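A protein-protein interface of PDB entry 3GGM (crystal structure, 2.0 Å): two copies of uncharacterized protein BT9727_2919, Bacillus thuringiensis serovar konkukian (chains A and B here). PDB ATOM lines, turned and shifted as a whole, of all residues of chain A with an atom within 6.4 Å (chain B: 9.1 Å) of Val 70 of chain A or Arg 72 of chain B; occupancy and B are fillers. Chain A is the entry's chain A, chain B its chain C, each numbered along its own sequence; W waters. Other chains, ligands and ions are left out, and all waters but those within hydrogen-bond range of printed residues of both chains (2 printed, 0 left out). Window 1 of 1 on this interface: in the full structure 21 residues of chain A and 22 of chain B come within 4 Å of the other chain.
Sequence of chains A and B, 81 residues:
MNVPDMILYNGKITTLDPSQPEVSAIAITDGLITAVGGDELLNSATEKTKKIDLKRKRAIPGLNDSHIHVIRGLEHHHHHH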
ATOM      1  N   ILE A  60      -8.465  -9.443   1.037  1.00  0.00           N
ATOM      2  CA  ILE A  60      -9.609  -8.540   0.960  1.00  0.00           C
ATOM      3  C   ILE A  60     -10.626  -9.032  -0.084  1.00  0.00           C
ATOM      4  O   ILE A  60     -10.251  -9.520  -1.151  1.00  0.00           O
ATOM      5  CB  ILE A  60      -9.129  -7.115   0.588  1.00  0.00           C
ATOM      6  CG1 ILE A  60      -7.976  -6.708   1.511  1.00  0.00           C
ATOM      7  CG2 ILE A  60     -10.263  -6.125   0.739  1.00  0.00           C
ATOM      8  CD1 ILE A  60      -7.220  -5.463   1.065  1.00  0.00           C
ATOM      9  N   PRO A  61     -11.927  -8.932   0.221  1.00  0.00           N
ATOM     10  CA  PRO A  61     -12.900  -9.399  -0.772  1.00  0.00           C
ATOM     11  C   PRO A  61     -12.794  -8.543  -2.041  1.00  0.00           C
ATOM     12  O   PRO A  61     -12.631  -7.334  -1.960  1.00  0.00           O
ATOM     13  CB  PRO A  61     -14.242  -9.209  -0.061  1.00  0.00           C
ATOM     14  CG  PRO A  61     -13.887  -9.277   1.414  1.00  0.00           C
ATOM     15  CD  PRO A  61     -12.606  -8.468   1.446  1.00  0.00           C
ATOM     16  N   GLY A  62     -12.867  -9.173  -3.207  1.00  0.00           N
ATOM     17  CA  GLY A  62     -12.801  -8.409  -4.449  1.00  0.00           C
ATOM     18  C   GLY A  62     -14.095  -7.631  -4.656  1.00  0.00           C
ATOM     19  O   GLY A  62     -15.124  -7.965  -4.059  1.00  0.00           O
ATOM     20  N   LEU A  63     -14.051  -6.578  -5.468  1.00  0.00           N
ATOM     21  CA  LEU A  63     -15.253  -5.796  -5.738  1.00  0.00           C
ATOM     22  C   LEU A  63     -16.269  -6.770  -6.306  1.00  0.00           C
ATOM     23  O   LEU A  63     -15.984  -7.504  -7.252  1.00  0.00           O
ATOM     24  CB  LEU A  63     -14.981  -4.679  -6.748  1.00  0.00           C
ATOM     25  CG  LEU A  63     -14.080  -3.517  -6.316  1.00  0.00           C
ATOM     26  CD1 LEU A  63     -14.527  -2.988  -4.949  1.00  0.00           C
ATOM     27  CD2 LEU A  63     -12.635  -3.997  -6.257  1.00  0.00           C
ATOM     28  N   ASN A  64     -17.457  -6.764  -5.720  1.00  0.00           N
ATOM     29  CA  ASN A  64     -18.516  -7.674  -6.111  1.00  0.00           C
ATOM     30  C   ASN A  64     -19.857  -6.939  -6.216  1.00  0.00           C
ATOM     31  O   ASN A  64     -20.654  -6.928  -5.275  1.00  0.00           O
ATOM     32  CB  ASN A  64     -18.578  -8.790  -5.063  1.00  0.00           C
ATOM     33  CG  ASN A  64     -19.662  -9.801  -5.337  1.00  0.00           C
ATOM     34  OD1 ASN A  64     -20.121  -9.952  -6.471  1.00  0.00           O
ATOM     35  ND2 ASN A  64     -20.063 -10.526  -4.297  1.00  0.00           N
ATOM     36  N   ILE A  68     -20.147  -2.705 -11.177  1.00  0.00           N
ATOM     37  CA  ILE A  68     -18.705  -2.546 -11.232  1.00  0.00           C
ATOM     38  C   ILE A  68     -18.041  -3.673 -12.013  1.00  0.00           C
ATOM     39  O   ILE A  68     -18.419  -4.833 -11.886  1.00  0.00           O
ATOM     40  CB  ILE A  68     -18.083  -2.549  -9.806  1.00  0.00           C
ATOM     41  CG1 ILE A  68     -18.756  -1.488  -8.919  1.00  0.00           C
ATOM     42  CG2 ILE A  68     -16.586  -2.298  -9.892  1.00  0.00           C
ATOM     43  CD1 ILE A  68     -18.467  -0.064  -9.318  1.00  0.00           C
ATOM     44  N   HIS A  69     -17.054  -3.320 -12.826  1.00  0.00           N
ATOM     45  CA  HIS A  69     -16.300  -4.310 -13.570  1.00  0.00           C
ATOM     46  C   HIS A  69     -14.856  -4.159 -13.120  1.00  0.00           C
ATOM     47  O   HIS A  69     -14.268  -3.086 -13.270  1.00  0.00           O
ATOM     48  CB  HIS A  69     -16.352  -4.068 -15.076  1.00  0.00           C
ATOM     49  CG  HIS A  69     -15.462  -4.997 -15.848  1.00  0.00           C
ATOM     50  ND1 HIS A  69     -15.908  -6.184 -16.384  1.00  0.00           N
ATOM     51  CD2 HIS A  69     -14.128  -4.952 -16.087  1.00  0.00           C
ATOM     52  CE1 HIS A  69     -14.888  -6.834 -16.917  1.00  0.00           C
ATOM     53  NE2 HIS A  69     -13.797  -6.108 -16.750  1.00  0.00           N
ATOM     54  N   VAL A  70     -14.288  -5.216 -12.555  1.00  0.00           N
ATOM     55  CA  VAL A  70     -12.892  -5.163 -12.125  1.00  0.00           C
ATOM     56  C   VAL A  70     -12.055  -5.510 -13.346  1.00  0.00           C
ATOM     57  O   VAL A  70     -12.230  -6.579 -13.921  1.00  0.00           O
ATOM     58  CB  VAL A  70     -12.598  -6.201 -11.021  1.00  0.00           C
ATOM     59  CG1 VAL A  70     -11.178  -5.984 -10.461  1.00  0.00           C
ATOM     60  CG2 VAL A  70     -13.638  -6.086  -9.917  1.00  0.00           C
ATOM     61  N   ILE A  71     -11.166  -4.612 -13.753  1.00  0.00           N
ATOM     62  CA  ILE A  71     -10.319  -4.863 -14.925  1.00  0.00           C
ATOM     63  C   ILE A  71      -9.211  -5.843 -14.552  1.00  0.00           C
ATOM     64  O   ILE A  71      -8.332  -5.525 -13.750  1.00  0.00           O
ATOM     65  CB  ILE A  71      -9.688  -3.561 -15.441  1.00  0.00           C
ATOM     66  CG1 ILE A  71     -10.783  -2.519 -15.683  1.00  0.00           C
ATOM     67  CG2 ILE A  71      -8.921  -3.833 -16.725  1.00  0.00           C
ATOM     68  CD1 ILE A  71     -10.248  -1.120 -16.024  1.00  0.00           C
ATOM     69  N   ARG A  72      -9.259  -7.032 -15.138  1.00  0.00           N
ATOM     70  CA  ARG A  72      -8.277  -8.079 -14.851  1.00  0.00           C
ATOM     71  C   ARG A  72      -7.108  -8.160 -15.837  1.00  0.00           C
ATOM     72  O   ARG A  72      -7.203  -7.718 -16.983  1.00  0.00           O
ATOM     73  CB  ARG A  72      -8.981  -9.442 -14.816  1.00  0.00           C
ATOM     74  CG  ARG A  72     -10.186  -9.510 -13.875  1.00  0.00           C
ATOM     75  CD  ARG A  72      -9.761  -9.254 -12.428  1.00  0.00           C
ATOM     76  NE  ARG A  72      -8.849 -10.292 -11.940  1.00  0.00           N
ATOM     77  CZ  ARG A  72      -9.224 -11.506 -11.563  1.00  0.00           C
ATOM     78  NH1 ARG A  72     -10.505 -11.849 -11.606  1.00  0.00           N
ATOM     79  NH2 ARG A  72      -8.319 -12.389 -11.158  1.00  0.00           N
ATOM     80  N   MET B   6      -6.916  -6.717 -26.448  1.00  0.00           N
ATOM     81  CA  MET B   6      -8.250  -6.545 -25.882  1.00  0.00           C
ATOM     82  C   MET B   6      -8.674  -5.091 -25.765  1.00  0.00           C
ATOM     83  O   MET B   6      -7.842  -4.200 -25.544  1.00  0.00           O
ATOM     84  CB  MET B   6      -8.282  -7.231 -24.492  1.00  0.00           C
ATOM     85  CG  MET B   6      -9.645  -7.264 -23.758  1.00  0.00           C
ATOM     86  SD  MET B   6      -9.607  -8.273 -22.192  1.00  0.00           S
ATOM     87  CE  MET B   6      -9.716  -9.890 -22.864  1.00  0.00           C
ATOM     88  N   LEU B   8     -11.785  -2.857 -23.830  1.00  0.00           N
ATOM     89  CA  LEU B   8     -12.951  -2.835 -22.967  1.00  0.00           C
ATOM     90  C   LEU B   8     -13.594  -1.497 -23.310  1.00  0.00           C
ATOM     91  O   LEU B   8     -12.949  -0.458 -23.200  1.00  0.00           O
ATOM     92  CB  LEU B   8     -12.530  -2.918 -21.487  1.00  0.00           C
ATOM     93  CG  LEU B   8     -11.603  -4.083 -21.097  1.00  0.00           C
ATOM     94  CD1 LEU B   8     -11.498  -4.147 -19.572  1.00  0.00           C
ATOM     95  CD2 LEU B   8     -12.144  -5.408 -21.625  1.00  0.00           C
ATOM     96  N   ILE B  28      -5.868  -2.912 -24.213  1.00  0.00           N
ATOM     97  CA  ILE B  28      -4.844  -3.676 -23.505  1.00  0.00           C
ATOM     98  C   ILE B  28      -3.984  -4.476 -24.477  1.00  0.00           C
ATOM     99  O   ILE B  28      -4.507  -5.177 -25.341  1.00  0.00           O
ATOM    100  CB  ILE B  28      -5.491  -4.670 -22.508  1.00  0.00           C
ATOM    101  CG1 ILE B  28      -6.329  -3.908 -21.480  1.00  0.00           C
ATOM    102  CG2 ILE B  28      -4.420  -5.497 -21.815  1.00  0.00           C
ATOM    103  CD1 ILE B  28      -7.125  -4.825 -20.529  1.00  0.00           C
ATOM    104  N   ILE B  52     -14.850  -6.283 -25.461  1.00  0.00           N
ATOM    105  CA  ILE B  52     -15.808  -6.536 -24.393  1.00  0.00           C
ATOM    106  C   ILE B  52     -16.623  -5.292 -24.051  1.00  0.00           C
ATOM    107  O   ILE B  52     -16.073  -4.236 -23.695  1.00  0.00           O
ATOM    108  CB  ILE B  52     -15.104  -7.018 -23.104  1.00  0.00           C
ATOM    109  CG1 ILE B  52     -14.373  -8.335 -23.371  1.00  0.00           C
ATOM    110  CG2 ILE B  52     -16.135  -7.191 -21.981  1.00  0.00           C
ATOM    111  CD1 ILE B  52     -13.375  -8.707 -22.298  1.00  0.00           C
ATOM    112  N   LEU B  54     -18.606  -3.189 -21.713  1.00  0.00           N
ATOM    113  CA  LEU B  54     -18.700  -3.011 -20.267  1.00  0.00           C
ATOM    114  C   LEU B  54     -20.116  -2.722 -19.781  1.00  0.00           C
ATOM    115  O   LEU B  54     -20.368  -2.685 -18.583  1.00  0.00           O
ATOM    116  CB  LEU B  54     -17.776  -1.881 -19.832  1.00  0.00           C
ATOM    117  CG  LEU B  54     -16.290  -2.187 -20.007  1.00  0.00           C
ATOM    118  CD1 LEU B  54     -15.491  -0.920 -19.813  1.00  0.00           C
ATOM    119  CD2 LEU B  54     -15.861  -3.267 -18.999  1.00  0.00           C
ATOM    120  N   LYS B  57     -20.864  -0.103 -17.008  1.00  0.00           N
ATOM    121  CA  LYS B  57     -20.326  -0.352 -15.681  1.00  0.00           C
ATOM    122  C   LYS B  57     -19.112   0.520 -15.449  1.00  0.00           C
ATOM    123  O   LYS B  57     -18.413   0.911 -16.392  1.00  0.00           O
ATOM    124  CB  LYS B  57     -19.867  -1.810 -15.534  1.00  0.00           C
ATOM    125  CG  LYS B  57     -20.953  -2.868 -15.502  1.00  0.00           C
ATOM    126  CD  LYS B  57     -20.320  -4.241 -15.713  1.00  0.00           C
ATOM    127  CE  LYS B  57     -21.344  -5.345 -15.652  1.00  0.00           C
ATOM    128  NZ  LYS B  57     -22.495  -5.005 -16.525  1.00  0.00           N
ATOM    129  N   ARG B  58     -18.860   0.816 -14.181  1.00  0.00           N
ATOM    130  CA  ARG B  58     -17.675   1.565 -13.797  1.00  0.00           C
ATOM    131  C   ARG B  58     -16.562   0.505 -13.766  1.00  0.00           C
ATOM    132  O   ARG B  58     -16.660  -0.479 -13.026  1.00  0.00           O
ATOM    133  CB  ARG B  58     -17.875   2.168 -12.409  1.00  0.00           C
ATOM    134  CG  ARG B  58     -16.597   2.635 -11.740  1.00  0.00           C
ATOM    135  CD  ARG B  58     -16.889   3.624 -10.612  1.00  0.00           C
ATOM    136  NE  ARG B  58     -16.711   4.997 -11.078  1.00  0.00           N
ATOM    137  CZ  ARG B  58     -17.551   5.645 -11.875  1.00  0.00           C
ATOM    138  NH1 ARG B  58     -18.661   5.059 -12.300  1.00  0.00           N
ATOM    139  NH2 ARG B  58     -17.256   6.868 -12.289  1.00  0.00           N
ATOM    140  N   ALA B  59     -15.517   0.693 -14.569  1.00  0.00           N
ATOM    141  CA  ALA B  59     -14.423  -0.276 -14.630  1.00  0.00           C
ATOM    142  C   ALA B  59     -13.240   0.216 -13.818  1.00  0.00           C
ATOM    143  O   ALA B  59     -12.742   1.317 -14.030  1.00  0.00           O
ATOM    144  CB  ALA B  59     -14.004  -0.524 -16.093  1.00  0.00           C
ATOM    145  N   ILE B  60     -12.795  -0.624 -12.888  1.00  0.00           N
ATOM    146  CA  ILE B  60     -11.704  -0.281 -11.992  1.00  0.00           C
ATOM    147  C   ILE B  60     -10.569  -1.289 -12.083  1.00  0.00           C
ATOM    148  O   ILE B  60     -10.802  -2.490 -12.043  1.00  0.00           O
ATOM    149  CB  ILE B  60     -12.228  -0.240 -10.536  1.00  0.00           C
ATOM    150  CG1 ILE B  60     -13.371   0.776 -10.436  1.00  0.00           C
ATOM    151  CG2 ILE B  60     -11.098   0.116  -9.570  1.00  0.00           C
ATOM    152  CD1 ILE B  60     -14.049   0.808  -9.093  1.00  0.00           C
ATOM    153  N   PRO B  61      -9.318  -0.809 -12.199  1.00  0.00           N
ATOM    154  CA  PRO B  61      -8.200  -1.751 -12.285  1.00  0.00           C
ATOM    155  C   PRO B  61      -8.223  -2.656 -11.054  1.00  0.00           C
ATOM    156  O   PRO B  61      -8.581  -2.220  -9.965  1.00  0.00           O
ATOM    157  CB  PRO B  61      -6.977  -0.839 -12.300  1.00  0.00           C
ATOM    158  CG  PRO B  61      -7.511   0.442 -12.927  1.00  0.00           C
ATOM    159  CD  PRO B  61      -8.843   0.583 -12.245  1.00  0.00           C
ATOM    160  N   GLY B  62      -7.870  -3.922 -11.238  1.00  0.00           N
ATOM    161  CA  GLY B  62      -7.848  -4.836 -10.117  1.00  0.00           C
ATOM    162  C   GLY B  62      -6.736  -4.414  -9.176  1.00  0.00           C
ATOM    163  O   GLY B  62      -5.697  -3.920  -9.614  1.00  0.00           O
ATOM    164  N   LEU B  63      -6.959  -4.586  -7.882  1.00  0.00           N
ATOM    165  CA  LEU B  63      -5.960  -4.229  -6.890  1.00  0.00           C
ATOM    166  C   LEU B  63      -4.811  -5.229  -7.009  1.00  0.00           C
ATOM    167  O   LEU B  63      -4.990  -6.416  -6.735  1.00  0.00           O
ATOM    168  CB  LEU B  63      -6.565  -4.321  -5.489  1.00  0.00           C
ATOM    169  CG  LEU B  63      -5.928  -3.490  -4.369  1.00  0.00           C
ATOM    170  CD1 LEU B  63      -6.275  -4.147  -3.043  1.00  0.00           C
ATOM    171  CD2 LEU B  63      -4.415  -3.397  -4.535  1.00  0.00           C
ATOM    172  N   ASN B  64      -3.635  -4.772  -7.431  1.00  0.00           N
ATOM    173  CA  ASN B  64      -2.516  -5.698  -7.548  1.00  0.00           C
ATOM    174  C   ASN B  64      -1.278  -5.169  -6.826  1.00  0.00           C
ATOM    175  O   ASN B  64      -0.565  -4.285  -7.306  1.00  0.00           O
ATOM    176  CB  ASN B  64      -2.223  -6.021  -9.025  1.00  0.00           C
ATOM    177  CG  ASN B  64      -1.719  -4.829  -9.807  1.00  0.00           C
ATOM    178  OD1 ASN B  64      -2.280  -3.732  -9.732  1.00  0.00           O
ATOM    179  ND2 ASN B  64      -0.660  -5.042 -10.581  1.00  0.00           N
ATOM    180  N   ASP B  65      -1.058  -5.723  -5.639  1.00  0.00           N
ATOM    181  CA  ASP B  65       0.056  -5.349  -4.781  1.00  0.00           C
ATOM    182  C   ASP B  65       0.554  -6.663  -4.204  1.00  0.00           C
ATOM    183  O   ASP B  65      -0.246  -7.548  -3.871  1.00  0.00           O
ATOM    184  CB  ASP B  65      -0.442  -4.429  -3.659  1.00  0.00           C
ATOM    185  CG  ASP B  65       0.684  -3.724  -2.936  1.00  0.00           C
ATOM    186  OD1 ASP B  65       1.199  -2.721  -3.471  1.00  0.00           O
ATOM    187  OD2 ASP B  65       1.056  -4.170  -1.832  1.00  0.00           O
ATOM    188  N   ILE B  68      -1.091  -7.888  -0.975  1.00  0.00           N
ATOM    189  CA  ILE B  68      -2.537  -8.086  -0.921  1.00  0.00           C
ATOM    190  C   ILE B  68      -3.034  -9.255  -1.756  1.00  0.00           C
ATOM    191  O   ILE B  68      -2.600  -9.456  -2.887  1.00  0.00           O
ATOM    192  CB  ILE B  68      -3.289  -6.820  -1.415  1.00  0.00           C
ATOM    193  CG1 ILE B  68      -2.871  -5.594  -0.601  1.00  0.00           C
ATOM    194  CG2 ILE B  68      -4.793  -7.030  -1.325  1.00  0.00           C
ATOM    195  CD1 ILE B  68      -3.256  -5.656   0.843  1.00  0.00           C
ATOM    196  N   HIS B  69      -3.933 -10.044  -1.186  1.00  0.00           N
ATOM    197  CA  HIS B  69      -4.529 -11.135  -1.933  1.00  0.00           C
ATOM    198  C   HIS B  69      -5.997 -10.765  -2.031  1.00  0.00           C
ATOM    199  O   HIS B  69      -6.673 -10.605  -1.008  1.00  0.00           O
ATOM    200  CB  HIS B  69      -4.412 -12.481  -1.216  1.00  0.00           C
ATOM    201  CG  HIS B  69      -5.205 -13.571  -1.875  1.00  0.00           C
ATOM    202  ND1 HIS B  69      -4.665 -14.429  -2.805  1.00  0.00           N
ATOM    203  CD2 HIS B  69      -6.523 -13.877  -1.802  1.00  0.00           C
ATOM    204  CE1 HIS B  69      -5.615 -15.215  -3.282  1.00  0.00           C
ATOM    205  NE2 HIS B  69      -6.753 -14.900  -2.691  1.00  0.00           N
ATOM    206  N   VAL B  70      -6.484 -10.597  -3.254  1.00  0.00           N
ATOM    207  CA  VAL B  70      -7.883 -10.254  -3.458  1.00  0.00           C
ATOM    208  C   VAL B  70      -8.665 -11.551  -3.579  1.00  0.00           C
ATOM    209  O   VAL B  70      -8.410 -12.358  -4.468  1.00  0.00           O
ATOM    210  CB  VAL B  70      -8.083  -9.414  -4.748  1.00  0.00           C
ATOM    211  CG1 VAL B  70      -9.549  -9.024  -4.886  1.00  0.00           C
ATOM    212  CG2 VAL B  70      -7.213  -8.162  -4.702  1.00  0.00           C
ATOM    213  N   ILE B  71      -9.610 -11.756  -2.667  1.00  0.00           N
ATOM    214  CA  ILE B  71     -10.429 -12.954  -2.683  1.00  0.00           C
ATOM    215  C   ILE B  71     -11.424 -12.828  -3.829  1.00  0.00           C
ATOM    216  O   ILE B  71     -12.215 -11.887  -3.866  1.00  0.00           O
ATOM    217  CB  ILE B  71     -11.207 -13.117  -1.361  1.00  0.00           C
ATOM    218  CG1 ILE B  71     -10.231 -13.123  -0.178  1.00  0.00           C
ATOM    219  CG2 ILE B  71     -12.005 -14.414  -1.402  1.00  0.00           C
ATOM    220  CD1 ILE B  71     -10.880 -12.900   1.167  1.00  0.00           C
ATOM    221  N   ARG B  72     -11.382 -13.779  -4.755  1.00  0.00           N
ATOM    222  CA  ARG B  72     -12.277 -13.766  -5.910  1.00  0.00           C
ATOM    223  C   ARG B  72     -13.379 -14.815  -5.777  1.00  0.00           C
ATOM    224  O   ARG B  72     -14.379 -14.773  -6.497  1.00  0.00           O
ATOM    225  CB  ARG B  72     -11.482 -14.044  -7.196  1.00  0.00           C
ATOM    226  CG  ARG B  72     -10.381 -13.031  -7.529  1.00  0.00           C
ATOM    227  CD  ARG B  72     -10.947 -11.640  -7.801  1.00  0.00           C
ATOM    228  NE  ARG B  72      -9.888 -10.676  -8.092  1.00  0.00           N
ATOM    229  CZ  ARG B  72     -10.066  -9.359  -8.150  1.00  0.00           C
ATOM    230  NH1 ARG B  72     -11.265  -8.840  -7.940  1.00  0.00           N
ATOM    231  NH2 ARG B  72      -9.039  -8.558  -8.399  1.00  0.00           N
ATOM    232  N   GLY B  73     -13.200 -15.750  -4.853  1.00  0.00           N
ATOM    233  CA  GLY B  73     -14.179 -16.811  -4.684  1.00  0.00           C
ATOM    234  C   GLY B  73     -15.546 -16.491  -4.095  1.00  0.00           C
ATOM    235  O   GLY B  73     -16.387 -17.390  -3.995  1.00  0.00           O
ATOM    236  N   LEU B  74     -15.795 -15.243  -3.710  1.00  0.00           N
ATOM    237  CA  LEU B  74     -17.085 -14.905  -3.113  1.00  0.00           C
ATOM    238  C   LEU B  74     -18.138 -14.515  -4.136  1.00  0.00           C
ATOM    239  O   LEU B  74     -19.221 -15.139  -4.116  1.00  0.00           O
ATOM    240  CB  LEU B  74     -16.926 -13.781  -2.086  1.00  0.00           C
ATOM    241  CG  LEU B  74     -15.892 -14.041  -0.985  1.00  0.00           C
ATOM    242  CD1 LEU B  74     -15.939 -12.892   0.011  1.00  0.00           C
ATOM    243  CD2 LEU B  74     -16.166 -15.370  -0.283  1.00  0.00           C
HETATM  244  O   HOH W   1      -7.060 -11.230  -8.492  1.00  0.00           O
HETATM  245  O   HOH W   2     -14.271  -9.740  -7.404  1.00  0.00           O
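The backbone carbonyl oxygen of Gly 62 of chain B lies close to the side-chain amide oxygen of Asn 64 of chain B.
Ile 60 of chain A touches Ile 68 of chain B, but with the chains exchanged Ile 68 of chain A does not touch Ile 60 of chain B (4.1 Å).
Ile 60 of chain A touches Ile 71 of chain B, and with the chains exchanged Ile 71 of chain A touches Ile 60 of chain B.
Gly 62 of chain A touches Ile 71 of chain B, and with the chains exchanged Ile 71 of chain A touches Gly 62 of chain B.
Arg 72 of chain B touches its own counterpart, Arg 72 of chain A.
Of the 22 pairs that touch across the chains among the printed residues, 13 have their exchanged pair printed and touching as well.
Of the printed residues of chain B, Ile 60 of chain A touches Ile 68 (3.7 Å), His 69 (3.0 Å), Val 70 (3.4 Å) and Ile 71 (2.8 Å).
His 69 of chain A touches just these residues of chain B: Leu 54, Arg 58, Ala 59 and Ile 60.
Val 70 of chain A touches just these residues of chain B: Ile 60, Gly 62 and Arg 72.
Of the printed residues of chain B, Ile 71 of chain A touches Leu 8, Ala 59, Ile 60, Pro 61 and Gly 62.
Of the printed residues of chain A, Leu 8 of chain B touches Ile 71 (3.9 Å).
Arg 72 of chain B touches just these residues of chain A: Gly 62 (3.8 Å), Val 70 (3.8 Å) and Arg 72 (3.6 Å).
The nearest residue of chain B that does not touch Val 70 of chain A is Pro 61 of chain B (4.5 Å).
The nearest printed residue of chain A that does not touch Pro 61 of chain B is Val 70 of chain A (4.5 Å).
The backbone NH (N) of Ile 60 of chain A is in hydrogen-bond range of the backbone carbonyl oxygen (O) of His 69 of chain B.
The backbone carbonyl oxygen (O) of Ile 60 of chain A is in hydrogen-bond range of the backbone NH (N) of Ile 71 of chain B, 2.8 Å away.
The backbone carbonyl oxygen (O) of Ile 71 of chain B is in hydrogen-bond range of the backbone NH (N) of Gly 62 of chain A, 2.9 Å away.
The backbone NH (N) of His 69 of chain A is in hydrogen-bond range of the backbone carbonyl oxygen (O) of Arg 58 of chain B (2.9 Å).
O of His 69 of chain A is in hydrogen-bond range of N of Ile 60 of chain B.
The backbone NH (N) of Ile 71 of chain A is in hydrogen-bond range of the backbone carbonyl oxygen (O) of Ile 60 of chain B, at 2.7 Å.
The backbone NH (N) of Gly 62 of chain B lies within hydrogen-bond range of the backbone carbonyl oxygen (O) of Ile 71 of chain A, at 3.0 Å.
Hydrophobic or aromatic side chains of chain A that line the printed part of chain B: Ile 60, Ile 68, His 69, Val 70 and Ile 71.
Printed residues of chain B that touch a printed residue of chain A: Leu 8, Leu 54, Arg 58, Ala 59, Ile 60, Pro 61, Gly 62, Ile 68, His 69, Val 70, Ile 71 and Arg 72.
Hydrophobic or aromatic side chains of chain B within 4 Å of the printed part of chain A: Leu 8, Leu 54, Ala 59, Ile 68, Val 70 and Ile 71.
Among the printed residues, pairs that only touch across the chains: His 69 of chain A with Ala 59 of chain B (3.1 Å), Gly 62 of chain A with Val 70 of chain B (3.3 Å), Ile 60 of chain A with Val 70 of chain B (3.4 Å), Val 70 of chain A with Ile 60 of chain B (3.4 Å), Ile 68 of chain A with Arg 58 of chain B (3.4 Å), Val 70 of chain A with Gly 62 of chain B (3.5 Å), His 69 of chain A with Leu 54 of chain B (3.6 Å), Arg 72 of chain A with Arg 72 of chain B (3.6 Å), Ile 60 of chain A with Ile 68 of chain B (3.7 Å), Ile 71 of chain A with Ala 59 of chain B (3.8 Å), Val 70 of chain A with Arg 72 of chain B (3.8 Å), Gly 62 of chain A with Arg 72 of chain B (3.8 Å), Ile 71 of chain A with Leu 8 of chain B (3.9 Å), Pro 61 of chain A with Ile 71 of chain B (3.9 Å) and Ile 71 of chain A with Pro 61 of chain B (3.9 Å).
Water W2 bridges O of Leu 63 of chain A and NH1 of Arg 72 of chain B.
Water W1 bridges NE of Arg 72 of chain B (2.9 Å) and NH2 of Arg 72 of chain A (3.2 Å).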
